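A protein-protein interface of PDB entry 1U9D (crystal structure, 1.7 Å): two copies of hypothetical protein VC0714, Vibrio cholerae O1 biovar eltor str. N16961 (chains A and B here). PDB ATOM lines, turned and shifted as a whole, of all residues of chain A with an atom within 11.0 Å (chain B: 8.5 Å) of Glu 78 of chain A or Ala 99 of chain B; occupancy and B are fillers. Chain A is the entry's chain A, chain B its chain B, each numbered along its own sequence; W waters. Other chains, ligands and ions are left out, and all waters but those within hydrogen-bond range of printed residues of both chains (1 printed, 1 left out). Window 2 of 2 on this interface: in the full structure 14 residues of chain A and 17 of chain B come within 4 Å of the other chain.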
ATOM      1  N   SER A  12      22.730  -6.523  24.121  1.00  0.00           N
ATOM      2  CA  SER A  12      22.654  -5.517  25.196  1.00  0.00           C
ATOM      3  C   SER A  12      21.283  -4.831  25.171  1.00  0.00           C
ATOM      4  O   SER A  12      20.717  -4.434  26.213  1.00  0.00           O
ATOM      5  CB  SER A  12      23.830  -4.542  25.028  1.00  0.00           C
ATOM      6  OG  SER A  12      24.232  -3.966  26.256  1.00  0.00           O
ATOM      7  N   SER A  13      20.706  -4.763  23.974  1.00  0.00           N
ATOM      8  CA  SER A  13      19.396  -4.160  23.780  1.00  0.00           C
ATOM      9  C   SER A  13      18.287  -5.037  24.386  1.00  0.00           C
ATOM     10  O   SER A  13      17.185  -4.544  24.686  1.00  0.00           O
ATOM     11  CB  SER A  13      19.158  -3.901  22.285  1.00  0.00           C
ATOM     12  OG  SER A  13      19.197  -5.107  21.533  1.00  0.00           O
ATOM     13  N   ASN A  14      18.557  -6.333  24.557  1.00  0.00           N
ATOM     14  CA  ASN A  14      17.592  -7.253  25.164  1.00  0.00           C
ATOM     15  C   ASN A  14      17.735  -7.192  26.671  1.00  0.00           C
ATOM     16  O   ASN A  14      18.551  -7.918  27.267  1.00  0.00           O
ATOM     17  CB  ASN A  14      17.807  -8.698  24.722  1.00  0.00           C
ATOM     18  CG  ASN A  14      16.804  -9.674  25.385  1.00  0.00           C
ATOM     19  OD1 ASN A  14      15.847  -9.255  26.063  1.00  0.00           O
ATOM     20  ND2 ASN A  14      17.036 -10.970  25.213  1.00  0.00           N
ATOM     21  N   ALA A  15      16.949  -6.317  27.273  1.00  0.00           N
ATOM     22  CA  ALA A  15      17.007  -6.141  28.715  1.00  0.00           C
ATOM     23  C   ALA A  15      16.230  -7.203  29.514  1.00  0.00           C
ATOM     24  O   ALA A  15      16.239  -7.162  30.735  1.00  0.00           O
ATOM     25  CB  ALA A  15      16.517  -4.763  29.076  1.00  0.00           C
ATOM     26  N   LEU A  43       8.834  -1.182  20.199  1.00  0.00           N
ATOM     27  CA  LEU A  43       9.645  -0.078  20.673  1.00  0.00           C
ATOM     28  C   LEU A  43      11.092  -0.477  20.929  1.00  0.00           C
ATOM     29  O   LEU A  43      11.990   0.254  20.567  1.00  0.00           O
ATOM     30  CB  LEU A  43       9.060   0.494  21.943  1.00  0.00           C
ATOM     31  CG  LEU A  43       9.841   1.680  22.480  1.00  0.00           C
ATOM     32  CD1 LEU A  43       9.582   2.906  21.594  1.00  0.00           C
ATOM     33  CD2 LEU A  43       9.490   1.929  23.920  1.00  0.00           C
ATOM     34  N   LEU A  44      11.303  -1.630  21.552  1.00  0.00           N
ATOM     35  CA  LEU A  44      12.622  -2.058  22.000  1.00  0.00           C
ATOM     36  C   LEU A  44      13.307  -3.010  21.036  1.00  0.00           C
ATOM     37  O   LEU A  44      14.457  -3.397  21.267  1.00  0.00           O
ATOM     38  CB  LEU A  44      12.514  -2.700  23.373  1.00  0.00           C
ATOM     39  CG  LEU A  44      11.797  -1.781  24.355  1.00  0.00           C
ATOM     40  CD1 LEU A  44      11.623  -2.464  25.671  1.00  0.00           C
ATOM     41  CD2 LEU A  44      12.519  -0.414  24.527  1.00  0.00           C
ATOM     42  N   TRP A  74      14.850  -5.564  35.169  1.00  0.00           N
ATOM     43  CA  TRP A  74      15.501  -5.746  33.868  1.00  0.00           C
ATOM     44  C   TRP A  74      16.996  -5.547  33.917  1.00  0.00           C
ATOM     45  O   TRP A  74      17.505  -5.173  34.933  1.00  0.00           O
ATOM     46  CB  TRP A  74      14.858  -4.805  32.851  1.00  0.00           C
ATOM     47  CG  TRP A  74      15.187  -3.337  33.018  1.00  0.00           C
ATOM     48  CD1 TRP A  74      15.709  -2.704  34.119  1.00  0.00           C
ATOM     49  CD2 TRP A  74      14.987  -2.322  32.038  1.00  0.00           C
ATOM     50  NE1 TRP A  74      15.866  -1.361  33.863  1.00  0.00           N
ATOM     51  CE2 TRP A  74      15.434  -1.105  32.589  1.00  0.00           C
ATOM     52  CE3 TRP A  74      14.481  -2.323  30.734  1.00  0.00           C
ATOM     53  CZ2 TRP A  74      15.389   0.089  31.887  1.00  0.00           C
ATOM     54  CZ3 TRP A  74      14.442  -1.141  30.036  1.00  0.00           C
ATOM     55  CH2 TRP A  74      14.886   0.050  30.618  1.00  0.00           C
ATOM     56  N   PHE A  75      17.703  -5.778  32.816  1.00  0.00           N
ATOM     57  CA  PHE A  75      19.157  -5.530  32.795  1.00  0.00           C
ATOM     58  C   PHE A  75      19.553  -4.086  32.591  1.00  0.00           C
ATOM     59  O   PHE A  75      20.741  -3.731  32.722  1.00  0.00           O
ATOM     60  CB  PHE A  75      19.833  -6.356  31.695  1.00  0.00           C
ATOM     61  CG  PHE A  75      19.775  -7.831  31.918  1.00  0.00           C
ATOM     62  CD1 PHE A  75      20.010  -8.359  33.154  1.00  0.00           C
ATOM     63  CD2 PHE A  75      19.534  -8.701  30.853  1.00  0.00           C
ATOM     64  CE1 PHE A  75      19.984  -9.735  33.361  1.00  0.00           C
ATOM     65  CE2 PHE A  75      19.520 -10.077  31.046  1.00  0.00           C
ATOM     66  CZ  PHE A  75      19.722 -10.592  32.295  1.00  0.00           C
ATOM     67  N   GLY A  76      18.602  -3.241  32.223  1.00  0.00           N
ATOM     68  CA  GLY A  76      18.915  -1.839  32.051  1.00  0.00           C
ATOM     69  C   GLY A  76      18.978  -1.457  30.571  1.00  0.00           C
ATOM     70  O   GLY A  76      19.451  -2.211  29.715  1.00  0.00           O
ATOM     71  N   ARG A  77      18.410  -0.303  30.276  1.00  0.00           N
ATOM     72  CA  ARG A  77      18.681   0.422  29.046  1.00  0.00           C
ATOM     73  C   ARG A  77      19.022   1.860  29.460  1.00  0.00           C
ATOM     74  O   ARG A  77      18.802   2.278  30.620  1.00  0.00           O
ATOM     75  CB  ARG A  77      17.452   0.383  28.144  1.00  0.00           C
ATOM     76  CG  ARG A  77      17.086  -1.012  27.620  1.00  0.00           C
ATOM     77  CD  ARG A  77      17.961  -1.503  26.490  1.00  0.00           C
ATOM     78  NE  ARG A  77      17.777  -0.682  25.286  1.00  0.00           N
ATOM     79  CZ  ARG A  77      17.018  -0.972  24.248  1.00  0.00           C
ATOM     80  NH1 ARG A  77      16.329  -2.091  24.173  1.00  0.00           N
ATOM     81  NH2 ARG A  77      16.947  -0.119  23.234  1.00  0.00           N
ATOM     82  N   GLU A  78      19.571   2.629  28.526  1.00  0.00           N
ATOM     83  CA  GLU A  78      19.965   4.012  28.808  1.00  0.00           C
ATOM     84  C   GLU A  78      18.763   4.829  29.285  1.00  0.00           C
ATOM     85  O   GLU A  78      17.626   4.504  28.965  1.00  0.00           O
ATOM     86  CB  GLU A  78      20.557   4.655  27.538  1.00  0.00           C
ATOM     87  CG  GLU A  78      19.488   4.958  26.477  1.00  0.00           C
ATOM     88  CD  GLU A  78      20.072   5.325  25.118  1.00  0.00           C
ATOM     89  OE1 GLU A  78      19.790   6.440  24.609  1.00  0.00           O
ATOM     90  OE2 GLU A  78      20.830   4.508  24.553  1.00  0.00           O
ATOM     91  N   GLN A  79      19.018   5.898  30.036  1.00  0.00           N
ATOM     92  CA  GLN A  79      17.955   6.743  30.576  1.00  0.00           C
ATOM     93  C   GLN A  79      16.877   7.128  29.586  1.00  0.00           C
ATOM     94  O   GLN A  79      15.703   7.120  29.918  1.00  0.00           O
ATOM     95  CB  GLN A  79      18.530   8.043  31.144  1.00  0.00           C
ATOM     96  CG  GLN A  79      17.499   8.869  31.919  1.00  0.00           C
ATOM     97  CD  GLN A  79      17.145   8.257  33.271  1.00  0.00           C
ATOM     98  OE1 GLN A  79      18.017   7.750  33.981  1.00  0.00           O
ATOM     99  NE2 GLN A  79      15.874   8.274  33.607  1.00  0.00           N
ATOM    100  N   GLN A  80      17.271   7.525  28.377  1.00  0.00           N
ATOM    101  CA  GLN A  80      16.300   7.984  27.402  1.00  0.00           C
ATOM    102  C   GLN A  80      15.335   6.869  26.989  1.00  0.00           C
ATOM    103  O   GLN A  80      14.157   7.111  26.824  1.00  0.00           O
ATOM    104  CB  GLN A  80      16.992   8.541  26.150  1.00  0.00           C
ATOM    105  CG  GLN A  80      16.003   9.168  25.197  1.00  0.00           C
ATOM    106  CD  GLN A  80      15.073  10.119  25.916  1.00  0.00           C
ATOM    107  OE1 GLN A  80      15.545  11.001  26.647  1.00  0.00           O
ATOM    108  NE2 GLN A  80      13.751   9.940  25.737  1.00  0.00           N
ATOM    109  N   THR A  81      15.838   5.654  26.830  1.00  0.00           N
ATOM    110  CA  THR A  81      14.978   4.519  26.503  1.00  0.00           C
ATOM    111  C   THR A  81      14.046   4.167  27.654  1.00  0.00           C
ATOM    112  O   THR A  81      12.849   3.927  27.461  1.00  0.00           O
ATOM    113  CB  THR A  81      15.846   3.350  26.108  1.00  0.00           C
ATOM    114  OG1 THR A  81      16.645   3.750  24.985  1.00  0.00           O
ATOM    115  CG2 THR A  81      15.023   2.165  25.587  1.00  0.00           C
ATOM    116  N   GLN A  82      14.613   4.141  28.848  1.00  0.00           N
ATOM    117  CA  GLN A  82      13.862   3.903  30.070  1.00  0.00           C
ATOM    118  C   GLN A  82      12.713   4.902  30.174  1.00  0.00           C
ATOM    119  O   GLN A  82      11.591   4.554  30.468  1.00  0.00           O
ATOM    120  CB  GLN A  82      14.828   4.005  31.268  1.00  0.00           C
ATOM    121  CG  GLN A  82      14.202   3.818  32.637  1.00  0.00           C
ATOM    122  CD  GLN A  82      15.233   3.935  33.744  1.00  0.00           C
ATOM    123  OE1 GLN A  82      15.989   2.988  34.003  1.00  0.00           O
ATOM    124  NE2 GLN A  82      15.291   5.098  34.383  1.00  0.00           N
ATOM    125  N   ASP A  83      12.994   6.166  29.901  1.00  0.00           N
ATOM    126  CA  ASP A  83      11.953   7.183  29.926  1.00  0.00           C
ATOM    127  C   ASP A  83      10.816   6.903  28.943  1.00  0.00           C
ATOM    128  O   ASP A  83       9.656   7.154  29.255  1.00  0.00           O
ATOM    129  CB  ASP A  83      12.507   8.567  29.550  1.00  0.00           C
ATOM    130  CG  ASP A  83      13.524   9.119  30.526  1.00  0.00           C
ATOM    131  OD1 ASP A  83      13.708   8.650  31.680  1.00  0.00           O
ATOM    132  OD2 ASP A  83      14.230  10.104  30.182  1.00  0.00           O
ATOM    133  N   GLN A  84      11.150   6.435  27.738  1.00  0.00           N
ATOM    134  CA  GLN A  84      10.134   6.104  26.736  1.00  0.00           C
ATOM    135  C   GLN A  84       9.262   4.937  27.156  1.00  0.00           C
ATOM    136  O   GLN A  84       8.048   4.926  26.934  1.00  0.00           O
ATOM    137  CB  GLN A  84      10.802   5.803  25.391  1.00  0.00           C
ATOM    138  CG  GLN A  84      11.056   7.054  24.562  1.00  0.00           C
ATOM    139  CD  GLN A  84       9.959   7.257  23.547  1.00  0.00           C
ATOM    140  OE1 GLN A  84       9.913   6.558  22.516  1.00  0.00           O
ATOM    141  NE2 GLN A  84       9.035   8.163  23.850  1.00  0.00           N
ATOM    142  N   ILE A  85       9.885   3.946  27.786  1.00  0.00           N
ATOM    143  CA  ILE A  85       9.145   2.787  28.254  1.00  0.00           C
ATOM    144  C   ILE A  85       8.159   3.180  29.307  1.00  0.00           C
ATOM    145  O   ILE A  85       7.030   2.703  29.309  1.00  0.00           O
ATOM    146  CB  ILE A  85      10.079   1.695  28.792  1.00  0.00           C
ATOM    147  CG1 ILE A  85      10.952   1.142  27.688  1.00  0.00           C
ATOM    148  CG2 ILE A  85       9.252   0.566  29.426  1.00  0.00           C
ATOM    149  CD1 ILE A  85      12.163   0.420  28.206  1.00  0.00           C
ATOM    150  N   ALA A  86       8.606   4.001  30.248  1.00  0.00           N
ATOM    151  CA  ALA A  86       7.747   4.501  31.281  1.00  0.00           C
ATOM    152  C   ALA A  86       6.568   5.224  30.650  1.00  0.00           C
ATOM    153  O   ALA A  86       5.440   5.084  31.092  1.00  0.00           O
ATOM    154  CB  ALA A  86       8.513   5.432  32.192  1.00  0.00           C
ATOM    155  N   GLN A  87       6.826   6.001  29.616  1.00  0.00           N
ATOM    156  CA  GLN A  87       5.735   6.734  28.963  1.00  0.00           C
ATOM    157  C   GLN A  87       4.720   5.809  28.265  1.00  0.00           C
ATOM    158  O   GLN A  87       3.517   6.031  28.384  1.00  0.00           O
ATOM    159  CB  GLN A  87       6.276   7.805  28.025  1.00  0.00           C
ATOM    160  CG  GLN A  87       5.272   8.923  27.664  1.00  0.00           C
ATOM    161  CD  GLN A  87       4.797   9.719  28.886  1.00  0.00           C
ATOM    162  OE1 GLN A  87       5.554  10.532  29.432  1.00  0.00           O
ATOM    163  NE2 GLN A  87       3.553   9.469  29.327  1.00  0.00           N
ATOM    164  N   PHE A 107      11.884   1.048  37.813  1.00  0.00           N
ATOM    165  CA  PHE A 107      12.783   0.111  37.181  1.00  0.00           C
ATOM    166  C   PHE A 107      13.795  -0.362  38.219  1.00  0.00           C
ATOM    167  O   PHE A 107      14.347   0.438  38.952  1.00  0.00           O
ATOM    168  CB  PHE A 107      13.464   0.791  35.996  1.00  0.00           C
ATOM    169  CG  PHE A 107      12.530   1.147  34.880  1.00  0.00           C
ATOM    170  CD1 PHE A 107      12.430   0.349  33.757  1.00  0.00           C
ATOM    171  CD2 PHE A 107      11.760   2.294  34.932  1.00  0.00           C
ATOM    172  CE1 PHE A 107      11.550   0.683  32.738  1.00  0.00           C
ATOM    173  CE2 PHE A 107      10.894   2.620  33.919  1.00  0.00           C
ATOM    174  CZ  PHE A 107      10.793   1.797  32.809  1.00  0.00           C
ATOM    175  N   PRO A 109      17.288  -2.486  38.406  1.00  0.00           N
ATOM    176  CA  PRO A 109      18.369  -3.117  37.643  1.00  0.00           C
ATOM    177  C   PRO A 109      18.801  -4.461  38.225  1.00  0.00           C
ATOM    178  O   PRO A 109      18.995  -4.587  39.424  1.00  0.00           O
ATOM    179  CB  PRO A 109      19.506  -2.099  37.770  1.00  0.00           C
ATOM    180  CG  PRO A 109      19.286  -1.501  39.088  1.00  0.00           C
ATOM    181  CD  PRO A 109      17.790  -1.312  39.140  1.00  0.00           C
ATOM    182  N   ARG A 112      23.630  -8.700  34.890  1.00  0.00           N
ATOM    183  CA  ARG A 112      23.728  -9.839  33.999  1.00  0.00           C
ATOM    184  C   ARG A 112      24.558 -10.980  34.561  1.00  0.00           C
ATOM    185  O   ARG A 112      24.249 -12.123  34.278  1.00  0.00           O
ATOM    186  CB  ARG A 112      24.330  -9.414  32.662  1.00  0.00           C
ATOM    187  CG  ARG A 112      23.405  -8.630  31.788  1.00  0.00           C
ATOM    188  CD  ARG A 112      24.128  -8.013  30.551  1.00  0.00           C
ATOM    189  NE  ARG A 112      23.124  -7.353  29.718  1.00  0.00           N
ATOM    190  CZ  ARG A 112      22.406  -7.955  28.783  1.00  0.00           C
ATOM    191  NH1 ARG A 112      22.604  -9.234  28.475  1.00  0.00           N
ATOM    192  NH2 ARG A 112      21.491  -7.267  28.132  1.00  0.00           N
ATOM    193  N   THR B  90      26.600   5.603  12.853  1.00  0.00           N
ATOM    194  CA  THR B  90      26.331   5.630  14.262  1.00  0.00           C
ATOM    195  C   THR B  90      25.071   6.422  14.560  1.00  0.00           C
ATOM    196  O   THR B  90      24.199   5.927  15.252  1.00  0.00           O
ATOM    197  CB  THR B  90      27.554   6.208  15.000  1.00  0.00           C
ATOM    198  OG1 THR B  90      28.685   5.380  14.697  1.00  0.00           O
ATOM    199  CG2 THR B  90      27.376   6.086  16.501  1.00  0.00           C
ATOM    200  N   ASP B  91      24.968   7.613  13.990  1.00  0.00           N
ATOM    201  CA  ASP B  91      23.816   8.481  14.198  1.00  0.00           C
ATOM    202  C   ASP B  91      22.507   7.824  13.719  1.00  0.00           C
ATOM    203  O   ASP B  91      21.516   7.835  14.435  1.00  0.00           O
ATOM    204  CB  ASP B  91      24.083   9.873  13.574  1.00  0.00           C
ATOM    205  CG  ASP B  91      25.219  10.654  14.307  1.00  0.00           C
ATOM    206  OD1 ASP B  91      25.610  10.244  15.432  1.00  0.00           O
ATOM    207  OD2 ASP B  91      25.798  11.680  13.840  1.00  0.00           O
ATOM    208  N   ILE B  93      21.864   4.469  13.375  1.00  0.00           N
ATOM    209  CA  ILE B  93      21.589   3.382  14.305  1.00  0.00           C
ATOM    210  C   ILE B  93      21.056   3.917  15.659  1.00  0.00           C
ATOM    211  O   ILE B  93      20.163   3.320  16.238  1.00  0.00           O
ATOM    212  CB  ILE B  93      22.858   2.506  14.491  1.00  0.00           C
ATOM    213  CG1 ILE B  93      22.992   1.546  13.308  1.00  0.00           C
ATOM    214  CG2 ILE B  93      22.819   1.725  15.781  1.00  0.00           C
ATOM    215  CD1 ILE B  93      24.395   1.149  13.011  1.00  0.00           C
ATOM    216  N   ARG B  94      21.587   5.032  16.145  1.00  0.00           N
ATOM    217  CA  ARG B  94      21.127   5.606  17.424  1.00  0.00           C
ATOM    218  C   ARG B  94      19.653   5.984  17.378  1.00  0.00           C
ATOM    219  O   ARG B  94      18.922   5.852  18.371  1.00  0.00           O
ATOM    220  CB  ARG B  94      21.922   6.852  17.808  1.00  0.00           C
ATOM    221  CG  ARG B  94      23.404   6.637  17.975  1.00  0.00           C
ATOM    222  CD  ARG B  94      24.040   7.296  19.167  1.00  0.00           C
ATOM    223  NE  ARG B  94      24.933   6.397  19.899  1.00  0.00           N
ATOM    224  CZ  ARG B  94      25.994   6.801  20.601  1.00  0.00           C
ATOM    225  NH1 ARG B  94      26.310   8.091  20.689  1.00  0.00           N
ATOM    226  NH2 ARG B  94      26.741   5.912  21.235  1.00  0.00           N
ATOM    227  N   GLN B  95      19.216   6.458  16.221  1.00  0.00           N
ATOM    228  CA  GLN B  95      17.815   6.821  16.035  1.00  0.00           C
ATOM    229  C   GLN B  95      16.881   5.644  16.195  1.00  0.00           C
ATOM    230  O   GLN B  95      15.749   5.812  16.618  1.00  0.00           O
ATOM    231  CB  GLN B  95      17.602   7.482  14.675  1.00  0.00           C
ATOM    232  CG  GLN B  95      17.574   8.987  14.792  1.00  0.00           C
ATOM    233  CD  GLN B  95      17.859   9.685  13.484  1.00  0.00           C
ATOM    234  OE1 GLN B  95      17.014   9.689  12.588  1.00  0.00           O
ATOM    235  NE2 GLN B  95      19.051  10.281  13.365  1.00  0.00           N
ATOM    236  N   LEU B  96      17.352   4.447  15.870  1.00  0.00           N
ATOM    237  CA  LEU B  96      16.535   3.252  16.005  1.00  0.00           C
ATOM    238  C   LEU B  96      16.777   2.482  17.300  1.00  0.00           C
ATOM    239  O   LEU B  96      15.862   1.835  17.794  1.00  0.00           O
ATOM    240  CB  LEU B  96      16.755   2.342  14.802  1.00  0.00           C
ATOM    241  CG  LEU B  96      16.502   3.046  13.465  1.00  0.00           C
ATOM    242  CD1 LEU B  96      17.104   2.269  12.304  1.00  0.00           C
ATOM    243  CD2 LEU B  96      15.022   3.280  13.252  1.00  0.00           C
ATOM    244  N   LEU B  97      17.987   2.571  17.852  1.00  0.00           N
ATOM    245  CA  LEU B  97      18.405   1.746  18.999  1.00  0.00           C
ATOM    246  C   LEU B  97      18.691   2.507  20.297  1.00  0.00           C
ATOM    247  O   LEU B  97      18.836   1.888  21.354  1.00  0.00           O
ATOM    248  CB  LEU B  97      19.645   0.909  18.633  1.00  0.00           C
ATOM    249  CG  LEU B  97      19.401  -0.463  18.001  1.00  0.00           C
ATOM    250  CD1 LEU B  97      20.733  -1.074  17.574  1.00  0.00           C
ATOM    251  CD2 LEU B  97      18.660  -1.433  18.945  1.00  0.00           C
ATOM    252  N   GLY B  98      18.807   3.823  20.234  1.00  0.00           N
ATOM    253  CA  GLY B  98      19.106   4.614  21.418  1.00  0.00           C
ATOM    254  C   GLY B  98      20.305   5.520  21.252  1.00  0.00           C
ATOM    255  O   GLY B  98      21.345   5.096  20.744  1.00  0.00           O
ATOM    256  N   ALA B  99      20.163   6.763  21.712  1.00  0.00           N
ATOM    257  CA  ALA B  99      21.208   7.790  21.585  1.00  0.00           C
ATOM    258  C   ALA B  99      22.432   7.571  22.470  1.00  0.00           C
ATOM    259  O   ALA B  99      23.338   8.407  22.501  1.00  0.00           O
ATOM    260  CB  ALA B  99      20.616   9.187  21.847  1.00  0.00           C
ATOM    261  N   ASP B 100      22.458   6.446  23.173  1.00  0.00           N
ATOM    262  CA  ASP B 100      23.543   6.095  24.088  1.00  0.00           C
ATOM    263  C   ASP B 100      23.903   4.606  23.993  1.00  0.00           C
ATOM    264  O   ASP B 100      24.765   4.122  24.735  1.00  0.00           O
ATOM    265  CB  ASP B 100      23.138   6.468  25.530  1.00  0.00           C
ATOM    266  CG  ASP B 100      23.961   7.614  26.105  1.00  0.00           C
ATOM    267  OD1 ASP B 100      24.250   8.588  25.368  1.00  0.00           O
ATOM    268  OD2 ASP B 100      24.365   7.622  27.290  1.00  0.00           O
ATOM    269  N   SER B 101      23.237   3.884  23.087  1.00  0.00           N
ATOM    270  CA  SER B 101      23.636   2.532  22.710  1.00  0.00           C
ATOM    271  C   SER B 101      25.062   2.632  22.228  1.00  0.00           C
ATOM    272  O   SER B 101      25.519   3.735  21.956  1.00  0.00           O
ATOM    273  CB  SER B 101      22.720   1.987  21.610  1.00  0.00           C
ATOM    274  OG  SER B 101      22.642   2.894  20.520  1.00  0.00           O
ATOM    275  N   HIS B 102      25.774   1.512  22.126  1.00  0.00           N
ATOM    276  CA  HIS B 102      27.223   1.579  21.899  1.00  0.00           C
ATOM    277  C   HIS B 102      27.748   0.868  20.640  1.00  0.00           C
ATOM    278  O   HIS B 102      28.475  -0.118  20.707  1.00  0.00           O
ATOM    279  CB  HIS B 102      27.946   1.083  23.145  1.00  0.00           C
ATOM    280  CG  HIS B 102      27.761   1.981  24.325  1.00  0.00           C
ATOM    281  ND1 HIS B 102      28.036   3.332  24.272  1.00  0.00           N
ATOM    282  CD2 HIS B 102      27.284   1.740  25.569  1.00  0.00           C
ATOM    283  CE1 HIS B 102      27.761   3.879  25.444  1.00  0.00           C
ATOM    284  NE2 HIS B 102      27.302   2.936  26.247  1.00  0.00           N
ATOM    285  N   LEU B 103      27.433   1.427  19.494  1.00  0.00           N
ATOM    286  CA  LEU B 103      27.754   0.812  18.218  1.00  0.00           C
ATOM    287  C   LEU B 103      29.250   0.809  17.920  1.00  0.00           C
ATOM    288  O   LEU B 103      29.899   1.832  18.086  1.00  0.00           O
ATOM    289  CB  LEU B 103      27.062   1.593  17.106  1.00  0.00           C
ATOM    290  CG  LEU B 103      27.275   1.015  15.716  1.00  0.00           C
ATOM    291  CD1 LEU B 103      26.397  -0.205  15.534  1.00  0.00           C
ATOM    292  CD2 LEU B 103      26.990   2.056  14.662  1.00  0.00           C
HETATM  293  O   HOH W   1      14.296  -0.496  19.094  1.00  0.00           O
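Ala 15 of chain A touches none of the printed residues of chain B.
Printed residues of chain B within 4 Å of Arg 77 of chain A: Leu 97 (3.3 Å).
Glu 78 of chain A touches just these residues of chain B: Gly 98, Ala 99, Asp 100 and Ser 101.
No residue of chain A comes within 4 Å of Arg 94 of chain B.
Printed residues of chain A within 4 Å of Leu 97 of chain B: Arg 77 (3.3 Å).
Of chain A, only Glu 78 (3.5 Å) comes within 4 Å of Gly 98 of chain B.
Ala 99 of chain B touches just one residue of chain A: Glu 78 (2.9 Å).
Asp 100 of chain B touches just one residue of chain A: Glu 78.
Of chain A, only Glu 78 (2.9 Å) comes within 4 Å of Ser 101 of chain B.
The nearest residue of chain B that does not touch Glu 78 of chain A is Leu 97 of chain B (4.6 Å).
The nearest printed residue of chain A that does not touch Ala 99 of chain B is Gln 80 of chain A (5.7 Å).
The nearest printed residue of chain B that does not touch Arg 77 of chain A is Gly 98 of chain B (5.3 Å).
The backbone carbonyl oxygen (O) of Ser 13 of chain A lies within hydrogen-bond range of the guanidinium group (NH1) of Arg 77 of chain A.
The guanidinium group (NH1) of Arg 94 of chain B is in hydrogen-bond range of the backbone carbonyl oxygen (O) of Ala 99 of chain B (3.5 Å).
The backbone carbonyl oxygen (O) of Asp 100 of chain B sits close to a ring nitrogen (NE2) of His 102 of chain B, 3.2 Å away.
O of Gly 98 of chain B sits at hydrogen-bond distance from OG of Ser 101 of chain B, at 2.6 Å.
NH2 of Arg 94 of chain B lies within hydrogen-bond range of O of Ser 101 of chain B, at 2.6 Å.
Water W1 lies within hydrogen-bond range of O of Leu 43 of chain A (2.8 Å) and O of Leu 96 of chain B (3.1 Å).
No position is printed for both chains.
Printed residues of chain B that touch a printed residue of chain A: Leu 97, Gly 98, Ala 99, Asp 100 and Ser 101.
Of the 23 printed residues of chain A, 2 touch a printed residue of chain B.
Along chain A the printed residues that touch a printed residue of chain B span positions 77 to 78.
Among the printed residues, 5 pairs touch across the chains.
N of Ser 101 of chain B lies within hydrogen-bond range of OE2 of Glu 78 of chain A.
OE1 of Glu 78 of chain A is in hydrogen-bond range of N of Ala 99 of chain B, 2.9 Å away.
N of Asp 100 of chain B sits at hydrogen-bond distance from OE2 of Glu 78 of chain A (2.9 Å).
The guanidinium group of Arg 77 of chain A lies within hydrogen-bond range of the backbone carbonyl oxygen of Leu 97 of chain B (3.3 Å).
Among the printed residues, pairs that only touch across the chains: Glu 78 of chain A with Gly 98 of chain B.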
